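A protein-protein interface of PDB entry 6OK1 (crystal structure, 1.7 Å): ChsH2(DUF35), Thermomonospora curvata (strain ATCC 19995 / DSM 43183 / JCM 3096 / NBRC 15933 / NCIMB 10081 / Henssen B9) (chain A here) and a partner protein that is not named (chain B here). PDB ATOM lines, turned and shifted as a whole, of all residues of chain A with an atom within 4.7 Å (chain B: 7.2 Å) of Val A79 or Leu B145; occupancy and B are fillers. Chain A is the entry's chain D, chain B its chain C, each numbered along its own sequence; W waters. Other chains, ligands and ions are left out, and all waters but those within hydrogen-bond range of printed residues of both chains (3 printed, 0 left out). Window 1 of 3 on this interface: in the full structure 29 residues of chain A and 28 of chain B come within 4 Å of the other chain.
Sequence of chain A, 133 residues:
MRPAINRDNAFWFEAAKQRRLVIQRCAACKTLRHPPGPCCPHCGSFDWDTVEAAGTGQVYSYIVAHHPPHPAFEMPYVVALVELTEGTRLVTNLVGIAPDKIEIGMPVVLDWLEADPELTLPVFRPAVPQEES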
ATOM      1  N   SER A  61       4.950  -5.547  11.235  1.00  0.00           N
ATOM      2  CA  SER A  61       4.376  -4.533  12.104  1.00  0.00           C
ATOM      3  C   SER A  61       5.509  -3.629  12.569  1.00  0.00           C
ATOM      4  O   SER A  61       6.685  -3.884  12.295  1.00  0.00           O
ATOM      5  CB  SER A  61       3.631  -5.154  13.281  1.00  0.00           C
ATOM      6  OG  SER A  61       2.884  -4.159  13.953  1.00  0.00           O
ATOM      7  N   TYR A  62       5.145  -2.551  13.255  1.00  0.00           N
ATOM      8  CA  TYR A  62       6.173  -1.667  13.778  1.00  0.00           C
ATOM      9  C   TYR A  62       5.572  -0.740  14.832  1.00  0.00           C
ATOM     10  O   TYR A  62       4.354  -0.534  14.905  1.00  0.00           O
ATOM     11  CB  TYR A  62       6.848  -0.858  12.656  1.00  0.00           C
ATOM     12  CG  TYR A  62       5.924   0.160  12.078  1.00  0.00           C
ATOM     13  CD1 TYR A  62       4.960  -0.205  11.150  1.00  0.00           C
ATOM     14  CD2 TYR A  62       5.990   1.492  12.473  1.00  0.00           C
ATOM     15  CE1 TYR A  62       4.087   0.726  10.626  1.00  0.00           C
ATOM     16  CE2 TYR A  62       5.113   2.433  11.962  1.00  0.00           C
ATOM     17  CZ  TYR A  62       4.167   2.040  11.030  1.00  0.00           C
ATOM     18  OH  TYR A  62       3.273   2.948  10.511  1.00  0.00           O
ATOM     19  N   ILE A  63       6.460  -0.203  15.660  1.00  0.00           N
ATOM     20  CA  ILE A  63       6.105   0.792  16.662  1.00  0.00           C
ATOM     21  C   ILE A  63       7.028   1.990  16.511  1.00  0.00           C
ATOM     22  O   ILE A  63       8.165   1.866  16.051  1.00  0.00           O
ATOM     23  CB  ILE A  63       6.188   0.207  18.095  1.00  0.00           C
ATOM     24  CG1 ILE A  63       7.617  -0.220  18.453  1.00  0.00           C
ATOM     25  CG2 ILE A  63       5.255  -0.977  18.205  1.00  0.00           C
ATOM     26  CD1 ILE A  63       8.464   0.824  19.139  1.00  0.00           C
ATOM     27  N   TYR A  77      12.381   6.574  17.974  1.00  0.00           N
ATOM     28  CA  TYR A  77      13.017   5.532  17.186  1.00  0.00           C
ATOM     29  C   TYR A  77      11.972   4.486  16.844  1.00  0.00           C
ATOM     30  O   TYR A  77      10.865   4.499  17.382  1.00  0.00           O
ATOM     31  CB  TYR A  77      14.209   4.914  17.919  1.00  0.00           C
ATOM     32  CG  TYR A  77      13.872   4.232  19.222  1.00  0.00           C
ATOM     33  CD1 TYR A  77      13.857   4.950  20.412  1.00  0.00           C
ATOM     34  CD2 TYR A  77      13.603   2.865  19.271  1.00  0.00           C
ATOM     35  CE1 TYR A  77      13.574   4.340  21.617  1.00  0.00           C
ATOM     36  CE2 TYR A  77      13.329   2.232  20.480  1.00  0.00           C
ATOM     37  CZ  TYR A  77      13.316   2.982  21.656  1.00  0.00           C
ATOM     38  OH  TYR A  77      13.027   2.374  22.863  1.00  0.00           O
ATOM     39  N   VAL A  78      12.321   3.609  15.904  1.00  0.00           N
ATOM     40  CA  VAL A  78      11.397   2.632  15.348  1.00  0.00           C
ATOM     41  C   VAL A  78      11.909   1.245  15.674  1.00  0.00           C
ATOM     42  O   VAL A  78      13.095   0.950  15.492  1.00  0.00           O
ATOM     43  CB  VAL A  78      11.233   2.807  13.823  1.00  0.00           C
ATOM     44  CG1 VAL A  78      10.327   1.700  13.238  1.00  0.00           C
ATOM     45  CG2 VAL A  78      10.650   4.163  13.529  1.00  0.00           C
ATOM     46  N   VAL A  79      11.009   0.391  16.146  1.00  0.00           N
ATOM     47  CA  VAL A  79      11.255  -1.039  16.219  1.00  0.00           C
ATOM     48  C   VAL A  79      10.266  -1.729  15.300  1.00  0.00           C
ATOM     49  O   VAL A  79       9.052  -1.492  15.386  1.00  0.00           O
ATOM     50  CB  VAL A  79      11.130  -1.576  17.653  1.00  0.00           C
ATOM     51  CG1 VAL A  79      11.424  -3.072  17.686  1.00  0.00           C
ATOM     52  CG2 VAL A  79      12.040  -0.814  18.596  1.00  0.00           C
ATOM     53  N   ALA A  80      10.782  -2.578  14.424  1.00  0.00           N
ATOM     54  CA  ALA A  80       9.968  -3.277  13.446  1.00  0.00           C
ATOM     55  C   ALA A  80       9.925  -4.768  13.747  1.00  0.00           C
ATOM     56  O   ALA A  80      10.919  -5.352  14.189  1.00  0.00           O
ATOM     57  CB  ALA A  80      10.511  -3.055  12.034  1.00  0.00           C
ATOM     58  N   LEU A  81       8.773  -5.376  13.473  1.00  0.00           N
ATOM     59  CA  LEU A  81       8.632  -6.823  13.408  1.00  0.00           C
ATOM     60  C   LEU A  81       8.764  -7.176  11.937  1.00  0.00           C
ATOM     61  O   LEU A  81       7.876  -6.865  11.140  1.00  0.00           O
ATOM     62  CB  LEU A  81       7.293  -7.293  13.977  1.00  0.00           C
ATOM     63  CG  LEU A  81       6.983  -8.787  13.899  1.00  0.00           C
ATOM     64  CD1 LEU A  81       7.994  -9.616  14.696  1.00  0.00           C
ATOM     65  CD2 LEU A  81       5.527  -9.031  14.368  1.00  0.00           C
ATOM     66  N   VAL A  91      12.345  -9.257  15.493  1.00  0.00           N
ATOM     67  CA  VAL A  91      12.295  -7.891  15.987  1.00  0.00           C
ATOM     68  C   VAL A  91      13.665  -7.250  15.802  1.00  0.00           C
ATOM     69  O   VAL A  91      14.678  -7.787  16.256  1.00  0.00           O
ATOM     70  CB  VAL A  91      11.884  -7.870  17.472  1.00  0.00           C
ATOM     71  CG1 VAL A  91      11.995  -6.488  18.051  1.00  0.00           C
ATOM     72  CG2 VAL A  91      10.450  -8.389  17.609  1.00  0.00           C
ATOM     73  N   THR A  92      13.698  -6.098  15.144  1.00  0.00           N
ATOM     74  CA  THR A  92      14.919  -5.307  15.044  1.00  0.00           C
ATOM     75  C   THR A  92      14.523  -3.844  14.933  1.00  0.00           C
ATOM     76  O   THR A  92      13.341  -3.503  14.862  1.00  0.00           O
ATOM     77  CB  THR A  92      15.779  -5.663  13.817  1.00  0.00           C
ATOM     78  OG1 THR A  92      15.200  -5.047  12.672  1.00  0.00           O
ATOM     79  CG2 THR A  92      15.863  -7.154  13.581  1.00  0.00           C
ATOM     80  N   ASN A  93      15.525  -2.976  14.853  1.00  0.00           N
ATOM     81  CA  ASN A  93      15.232  -1.590  14.544  1.00  0.00           C
ATOM     82  C   ASN A  93      15.094  -1.410  13.045  1.00  0.00           C
ATOM     83  O   ASN A  93      15.556  -2.222  12.245  1.00  0.00           O
ATOM     84  CB  ASN A  93      16.317  -0.665  15.093  1.00  0.00           C
ATOM     85  CG  ASN A  93      16.417  -0.729  16.611  1.00  0.00           C
ATOM     86  OD1 ASN A  93      17.416  -1.202  17.151  1.00  0.00           O
ATOM     87  ND2 ASN A  93      15.384  -0.254  17.301  1.00  0.00           N
ATOM     88  N   TYR B 137      14.400 -11.836  27.002  1.00  0.00           N
ATOM     89  CA  TYR B 137      14.636 -10.407  26.824  1.00  0.00           C
ATOM     90  C   TYR B 137      15.705 -10.123  25.774  1.00  0.00           C
ATOM     91  O   TYR B 137      15.817  -8.976  25.313  1.00  0.00           O
ATOM     92  CB  TYR B 137      15.031  -9.781  28.170  1.00  0.00           C
ATOM     93  CG  TYR B 137      13.840  -9.572  29.094  1.00  0.00           C
ATOM     94  CD1 TYR B 137      12.986  -8.492  28.932  1.00  0.00           C
ATOM     95  CD2 TYR B 137      13.571 -10.467  30.112  1.00  0.00           C
ATOM     96  CE1 TYR B 137      11.887  -8.311  29.776  1.00  0.00           C
ATOM     97  CE2 TYR B 137      12.484 -10.288  30.959  1.00  0.00           C
ATOM     98  CZ  TYR B 137      11.647  -9.213  30.787  1.00  0.00           C
ATOM     99  OH  TYR B 137      10.556  -9.042  31.627  1.00  0.00           O
ATOM    100  N   TRP B 139      15.709 -10.791  22.769  1.00  0.00           N
ATOM    101  CA  TRP B 139      15.070 -10.433  21.502  1.00  0.00           C
ATOM    102  C   TRP B 139      14.430  -9.048  21.541  1.00  0.00           C
ATOM    103  O   TRP B 139      13.885  -8.593  20.522  1.00  0.00           O
ATOM    104  CB  TRP B 139      14.046 -11.517  21.126  1.00  0.00           C
ATOM    105  CG  TRP B 139      14.740 -12.827  21.201  1.00  0.00           C
ATOM    106  CD1 TRP B 139      14.520 -13.834  22.104  1.00  0.00           C
ATOM    107  CD2 TRP B 139      15.849 -13.242  20.399  1.00  0.00           C
ATOM    108  NE1 TRP B 139      15.428 -14.845  21.906  1.00  0.00           N
ATOM    109  CE2 TRP B 139      16.256 -14.506  20.867  1.00  0.00           C
ATOM    110  CE3 TRP B 139      16.551 -12.659  19.341  1.00  0.00           C
ATOM    111  CZ2 TRP B 139      17.324 -15.203  20.309  1.00  0.00           C
ATOM    112  CZ3 TRP B 139      17.626 -13.367  18.779  1.00  0.00           C
ATOM    113  CH2 TRP B 139      17.993 -14.623  19.270  1.00  0.00           C
ATOM    114  N   LEU B 140      14.508  -8.364  22.682  1.00  0.00           N
ATOM    115  CA  LEU B 140      13.741  -7.146  22.909  1.00  0.00           C
ATOM    116  C   LEU B 140      14.638  -5.987  23.310  1.00  0.00           C
ATOM    117  O   LEU B 140      14.644  -4.939  22.655  1.00  0.00           O
ATOM    118  CB  LEU B 140      12.688  -7.377  24.001  1.00  0.00           C
ATOM    119  CG  LEU B 140      11.810  -8.615  23.798  1.00  0.00           C
ATOM    120  CD1 LEU B 140      10.884  -8.810  25.010  1.00  0.00           C
ATOM    121  CD2 LEU B 140      10.977  -8.503  22.498  1.00  0.00           C
ATOM    122  N   LEU B 141      15.390  -6.157  24.389  1.00  0.00           N
ATOM    123  CA  LEU B 141      16.104  -5.028  24.962  1.00  0.00           C
ATOM    124  C   LEU B 141      17.182  -4.464  24.039  1.00  0.00           C
ATOM    125  O   LEU B 141      17.371  -3.242  24.015  1.00  0.00           O
ATOM    126  CB  LEU B 141      16.717  -5.425  26.309  1.00  0.00           C
ATOM    127  CG  LEU B 141      15.651  -5.944  27.292  1.00  0.00           C
ATOM    128  CD1 LEU B 141      16.287  -6.220  28.666  1.00  0.00           C
ATOM    129  CD2 LEU B 141      14.437  -5.006  27.421  1.00  0.00           C
ATOM    130  N   PRO B 142      17.909  -5.284  23.274  1.00  0.00           N
ATOM    131  CA  PRO B 142      18.967  -4.717  22.416  1.00  0.00           C
ATOM    132  C   PRO B 142      18.427  -3.767  21.365  1.00  0.00           C
ATOM    133  O   PRO B 142      19.185  -2.943  20.830  1.00  0.00           O
ATOM    134  CB  PRO B 142      19.612  -5.955  21.773  1.00  0.00           C
ATOM    135  CG  PRO B 142      19.340  -7.068  22.770  1.00  0.00           C
ATOM    136  CD  PRO B 142      17.964  -6.757  23.317  1.00  0.00           C
ATOM    137  N   PHE B 143      17.137  -3.868  21.052  1.00  0.00           N
ATOM    138  CA  PHE B 143      16.485  -3.056  20.041  1.00  0.00           C
ATOM    139  C   PHE B 143      15.625  -1.961  20.665  1.00  0.00           C
ATOM    140  O   PHE B 143      14.952  -1.226  19.941  1.00  0.00           O
ATOM    141  CB  PHE B 143      15.652  -3.975  19.139  1.00  0.00           C
ATOM    142  CG  PHE B 143      16.425  -5.175  18.652  1.00  0.00           C
ATOM    143  CD1 PHE B 143      17.385  -5.036  17.657  1.00  0.00           C
ATOM    144  CD2 PHE B 143      16.240  -6.424  19.222  1.00  0.00           C
ATOM    145  CE1 PHE B 143      18.122  -6.128  17.215  1.00  0.00           C
ATOM    146  CE2 PHE B 143      16.975  -7.521  18.794  1.00  0.00           C
ATOM    147  CZ  PHE B 143      17.924  -7.376  17.789  1.00  0.00           C
ATOM    148  N   GLY B 144      15.656  -1.811  21.983  1.00  0.00           N
ATOM    149  CA  GLY B 144      14.892  -0.755  22.605  1.00  0.00           C
ATOM    150  C   GLY B 144      13.409  -1.032  22.694  1.00  0.00           C
ATOM    151  O   GLY B 144      12.625  -0.097  22.863  1.00  0.00           O
ATOM    152  N   LEU B 145      12.997  -2.291  22.576  1.00  0.00           N
ATOM    153  CA  LEU B 145      11.599  -2.671  22.761  1.00  0.00           C
ATOM    154  C   LEU B 145      11.465  -3.132  24.202  1.00  0.00           C
ATOM    155  O   LEU B 145      11.408  -4.328  24.503  1.00  0.00           O
ATOM    156  CB  LEU B 145      11.197  -3.755  21.782  1.00  0.00           C
ATOM    157  CG  LEU B 145       9.686  -3.922  21.612  1.00  0.00           C
ATOM    158  CD1 LEU B 145       9.104  -2.719  20.834  1.00  0.00           C
ATOM    159  CD2 LEU B 145       9.317  -5.237  20.938  1.00  0.00           C
ATOM    160  N   ASN B 146      11.452  -2.165  25.113  1.00  0.00           N
ATOM    161  CA  ASN B 146      11.643  -2.501  26.509  1.00  0.00           C
ATOM    162  C   ASN B 146      10.463  -2.204  27.422  1.00  0.00           C
ATOM    163  O   ASN B 146      10.600  -2.413  28.632  1.00  0.00           O
ATOM    164  CB  ASN B 146      12.887  -1.795  27.061  1.00  0.00           C
ATOM    165  CG  ASN B 146      12.731  -0.303  27.132  1.00  0.00           C
ATOM    166  OD1 ASN B 146      12.104   0.290  26.277  1.00  0.00           O
ATOM    167  ND2 ASN B 146      13.331   0.317  28.141  1.00  0.00           N
ATOM    168  N   THR B 147       9.323  -1.731  26.905  1.00  0.00           N
ATOM    169  CA  THR B 147       8.187  -1.451  27.776  1.00  0.00           C
ATOM    170  C   THR B 147       6.935  -2.225  27.373  1.00  0.00           C
ATOM    171  O   THR B 147       6.746  -2.540  26.197  1.00  0.00           O
ATOM    172  CB  THR B 147       7.810   0.029  27.767  1.00  0.00           C
ATOM    173  OG1 THR B 147       7.212   0.344  26.507  1.00  0.00           O
ATOM    174  CG2 THR B 147       9.031   0.916  27.989  1.00  0.00           C
ATOM    175  N   PRO B 148       6.036  -2.486  28.330  1.00  0.00           N
ATOM    176  CA  PRO B 148       4.746  -3.124  27.995  1.00  0.00           C
ATOM    177  C   PRO B 148       3.951  -2.336  26.984  1.00  0.00           C
ATOM    178  O   PRO B 148       3.326  -2.931  26.097  1.00  0.00           O
ATOM    179  CB  PRO B 148       4.031  -3.200  29.349  1.00  0.00           C
ATOM    180  CG  PRO B 148       5.133  -3.199  30.361  1.00  0.00           C
ATOM    181  CD  PRO B 148       6.217  -2.343  29.786  1.00  0.00           C
ATOM    182  N   ALA B 149       3.948  -1.008  27.088  1.00  0.00           N
ATOM    183  CA  ALA B 149       3.228  -0.231  26.083  1.00  0.00           C
ATOM    184  C   ALA B 149       3.743  -0.539  24.682  1.00  0.00           C
ATOM    185  O   ALA B 149       2.957  -0.624  23.730  1.00  0.00           O
ATOM    186  CB  ALA B 149       3.344   1.262  26.377  1.00  0.00           C
ATOM    187  N   GLN B 150       5.065  -0.685  24.536  1.00  0.00           N
ATOM    188  CA  GLN B 150       5.659  -0.984  23.239  1.00  0.00           C
ATOM    189  C   GLN B 150       5.325  -2.397  22.788  1.00  0.00           C
ATOM    190  O   GLN B 150       5.027  -2.622  21.605  1.00  0.00           O
ATOM    191  CB  GLN B 150       7.172  -0.788  23.301  1.00  0.00           C
ATOM    192  CG  GLN B 150       7.580   0.657  23.440  1.00  0.00           C
ATOM    193  CD  GLN B 150       8.990   0.800  23.966  1.00  0.00           C
ATOM    194  OE1 GLN B 150       9.632  -0.194  24.289  1.00  0.00           O
ATOM    195  NE2 GLN B 150       9.478   2.041  24.068  1.00  0.00           N
ATOM    196  N   TRP B 151       5.353  -3.362  23.711  1.00  0.00           N
ATOM    197  CA  TRP B 151       4.978  -4.724  23.343  1.00  0.00           C
ATOM    198  C   TRP B 151       3.544  -4.771  22.836  1.00  0.00           C
ATOM    199  O   TRP B 151       3.245  -5.484  21.872  1.00  0.00           O
ATOM    200  CB  TRP B 151       5.181  -5.683  24.532  1.00  0.00           C
ATOM    201  CG  TRP B 151       6.587  -5.652  25.031  1.00  0.00           C
ATOM    202  CD1 TRP B 151       7.721  -5.400  24.284  1.00  0.00           C
ATOM    203  CD2 TRP B 151       7.044  -5.824  26.386  1.00  0.00           C
ATOM    204  NE1 TRP B 151       8.825  -5.421  25.085  1.00  0.00           N
ATOM    205  CE2 TRP B 151       8.447  -5.686  26.372  1.00  0.00           C
ATOM    206  CE3 TRP B 151       6.406  -6.111  27.598  1.00  0.00           C
ATOM    207  CZ2 TRP B 151       9.225  -5.780  27.537  1.00  0.00           C
ATOM    208  CZ3 TRP B 151       7.178  -6.216  28.751  1.00  0.00           C
ATOM    209  CH2 TRP B 151       8.575  -6.053  28.707  1.00  0.00           C
ATOM    210  N   VAL B 152       2.637  -4.019  23.469  1.00  0.00           N
ATOM    211  CA  VAL B 152       1.246  -4.016  23.030  1.00  0.00           C
ATOM    212  C   VAL B 152       1.114  -3.266  21.722  1.00  0.00           C
ATOM    213  O   VAL B 152       0.327  -3.652  20.845  1.00  0.00           O
ATOM    214  CB  VAL B 152       0.345  -3.406  24.119  1.00  0.00           C
ATOM    215  CG1 VAL B 152      -1.063  -3.142  23.589  1.00  0.00           C
ATOM    216  CG2 VAL B 152       0.294  -4.338  25.312  1.00  0.00           C
ATOM    217  N   ALA B 153       1.849  -2.163  21.589  1.00  0.00           N
ATOM    218  CA  ALA B 153       1.723  -1.322  20.399  1.00  0.00           C
ATOM    219  C   ALA B 153       1.981  -2.135  19.143  1.00  0.00           C
ATOM    220  O   ALA B 153       1.367  -1.891  18.094  1.00  0.00           O
ATOM    221  CB  ALA B 153       2.696  -0.149  20.489  1.00  0.00           C
ATOM    222  N   MET B 154       2.916  -3.087  19.218  1.00  0.00           N
ATOM    223  CA  MET B 154       3.249  -3.898  18.046  1.00  0.00           C
ATOM    224  C   MET B 154       2.032  -4.676  17.558  1.00  0.00           C
ATOM    225  O   MET B 154       1.826  -4.835  16.347  1.00  0.00           O
ATOM    226  CB  MET B 154       4.397  -4.845  18.383  1.00  0.00           C
ATOM    227  CG  MET B 154       5.013  -5.540  17.188  1.00  0.00           C
ATOM    228  SD  MET B 154       5.949  -4.402  16.174  1.00  0.00           S
ATOM    229  CE  MET B 154       7.456  -4.230  17.120  1.00  0.00           C
ATOM    230  N   VAL B 206       3.938   5.506  22.496  1.00  0.00           N
ATOM    231  CA  VAL B 206       4.518   4.693  21.441  1.00  0.00           C
ATOM    232  C   VAL B 206       3.397   4.474  20.437  1.00  0.00           C
ATOM    233  O   VAL B 206       2.351   3.915  20.785  1.00  0.00           O
ATOM    234  CB  VAL B 206       5.107   3.367  21.980  1.00  0.00           C
ATOM    235  CG1 VAL B 206       4.170   2.696  22.996  1.00  0.00           C
ATOM    236  CG2 VAL B 206       5.441   2.394  20.850  1.00  0.00           C
ATOM    237  N   THR B 257       4.883 -10.921  23.889  1.00  0.00           N
ATOM    238  CA  THR B 257       5.523 -10.722  22.589  1.00  0.00           C
ATOM    239  C   THR B 257       5.349 -11.921  21.651  1.00  0.00           C
ATOM    240  O   THR B 257       6.296 -12.339  20.982  1.00  0.00           O
ATOM    241  CB  THR B 257       7.009 -10.417  22.794  1.00  0.00           C
ATOM    242  OG1 THR B 257       7.665 -11.486  23.490  1.00  0.00           O
ATOM    243  CG2 THR B 257       7.191  -9.125  23.606  1.00  0.00           C
ATOM    244  N   TYR B 259       4.737 -12.666  18.680  1.00  0.00           N
ATOM    245  CA  TYR B 259       4.796 -12.024  17.374  1.00  0.00           C
ATOM    246  C   TYR B 259       5.039 -12.993  16.215  1.00  0.00           C
ATOM    247  O   TYR B 259       5.207 -12.537  15.077  1.00  0.00           O
ATOM    248  CB  TYR B 259       5.921 -10.994  17.379  1.00  0.00           C
ATOM    249  CG  TYR B 259       5.803  -9.868  18.388  1.00  0.00           C
ATOM    250  CD1 TYR B 259       4.551  -9.407  18.814  1.00  0.00           C
ATOM    251  CD2 TYR B 259       6.937  -9.264  18.909  1.00  0.00           C
ATOM    252  CE1 TYR B 259       4.456  -8.369  19.715  1.00  0.00           C
ATOM    253  CE2 TYR B 259       6.847  -8.233  19.819  1.00  0.00           C
ATOM    254  CZ  TYR B 259       5.605  -7.802  20.227  1.00  0.00           C
ATOM    255  OH  TYR B 259       5.546  -6.762  21.118  1.00  0.00           O
HETATM  256  O   HOH W   1      14.623  -9.847  18.102  1.00  0.00           O
HETATM  257  O   HOH W   2      12.014   2.990  25.359  1.00  0.00           O
HETATM  258  O   HOH W   3      19.632  -1.331  18.432  1.00  0.00           O
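Among the printed residues, merely in contact across the chains: Ile A63 with Leu B145 (3.8 Å), Ile A63 with Gln B150 (3.8 Å), Ile A63 with Ala B153 (3.5 Å), Ile A63 with Met B154 (3.3 Å), Ile A63 with Val B206 (3.6 Å), Tyr A77 with Phe B143 (3.9 Å), Tyr A77 with Gln B150 (3.8 Å), Val A79 with Phe B143 (3.2 Å), Val A79 with Leu B145 (3.9 Å), Val A79 with Met B154 (3.6 Å), Leu A81 with Met B154 (3.9 Å), Leu A81 with Tyr B259 (3.6 Å), Val A91 with Trp B139 (3.7 Å), Val A91 with Phe B143 (3.4 Å), Val A91 with Tyr B259 (3.8 Å) and Thr A92 with Phe B143 (3.6 Å).
Of the 20 printed residues of chain B, 9 touch a printed residue of chain A.
Printed residues of chain B that touch a printed residue of chain A: Trp B139, Phe B143, Gly B144, Leu B145, Gln B150, Ala B153, Met B154, Val B206 and Tyr B259.
Hydrophobic or aromatic side chains of chain B that line the printed part of chain A: Phe B143, Leu B145, Ala B153, Met B154, Val B206 and Tyr B259.
Of the 11 printed residues of chain A, 9 touch a printed residue of chain B.
Hydrophobic or aromatic side chains of chain A within 4 Å of the printed part of chain B: Ile A63, Tyr A77, Val A79, Leu A81 and Val A91.
The backbone carbonyl oxygen of Phe B143 lies within hydrogen-bond range of the side-chain amide nitrogen of Asn A93 (2.8 Å).
O of Gly B144 sits at hydrogen-bond distance from OH of Tyr A77 (2.5 Å).
The side-chain hydroxyl (OG) of Ser A61 is in hydrogen-bond range of the backbone carbonyl oxygen (O) of Met B154.
SD of Met B154 is in hydrogen-bond range of N of Tyr A62, at 3.5 Å.
Printed residues of chain B within 4 Å of Tyr A77: Phe B143, Gly B144 and Gln B150.
Val A79 touches just these residues of chain B: Phe B143, Leu B145 and Met B154.
Ala A80 touches none of the printed residues of chain B.
Leu B145 touches just these residues of chain A: Ile A63 and Val A79.
Val B152 touches none of the printed residues of chain A.
Printed residues of chain A within 4 Å of Met B154: Ser A61, Tyr A62, Ile A63, Val A79 and Leu A81.
The nearest residue of chain B that does not touch Val A79 is Gly B144 (4.3 Å).
The nearest residue of chain A that does not touch Leu B145 is Val A91 (4.1 Å).
The nearest printed residue of chain B that does not touch Asn A93 is Pro B142 (4.4 Å).
The side-chain amide oxygen (OD1) of Asn B146 sits close to the backbone carbonyl oxygen (O) of Gly B144, at 3.5 Å.
The side-chain amide oxygen (OE1) of Gln B150 lies close to the backbone carbonyl oxygen (O) of Gly B144 (3.3 Å).
OE1 of Gln B150 is in hydrogen-bond range of N of Asn B146 (2.8 Å).
The backbone NH (N) of Thr B147 is in hydrogen-bond range of the side-chain amide oxygen (OE1) of Gln B150 (3.0 Å).
The side-chain hydroxyl (OH) of Tyr B259 lies within hydrogen-bond range of the backbone carbonyl oxygen (O) of Trp B151 (2.7 Å).
O of Ser A61 sits at hydrogen-bond distance from N of Leu A81 (2.8 Å).
Water W3 lies within hydrogen-bond range of the side-chain amide oxygen of Asn A93 (2.6 Å) and the backbone carbonyl oxygen of Pro B142 (2.9 Å).
Water W2 lies within hydrogen-bond range of OH of Tyr A77 (2.8 Å), OD1 of Asn B146 (2.9 Å) and NE2 of Gln B150 (3.0 Å).
Water W1 bridges O of Val A91 and O of Trp B139.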
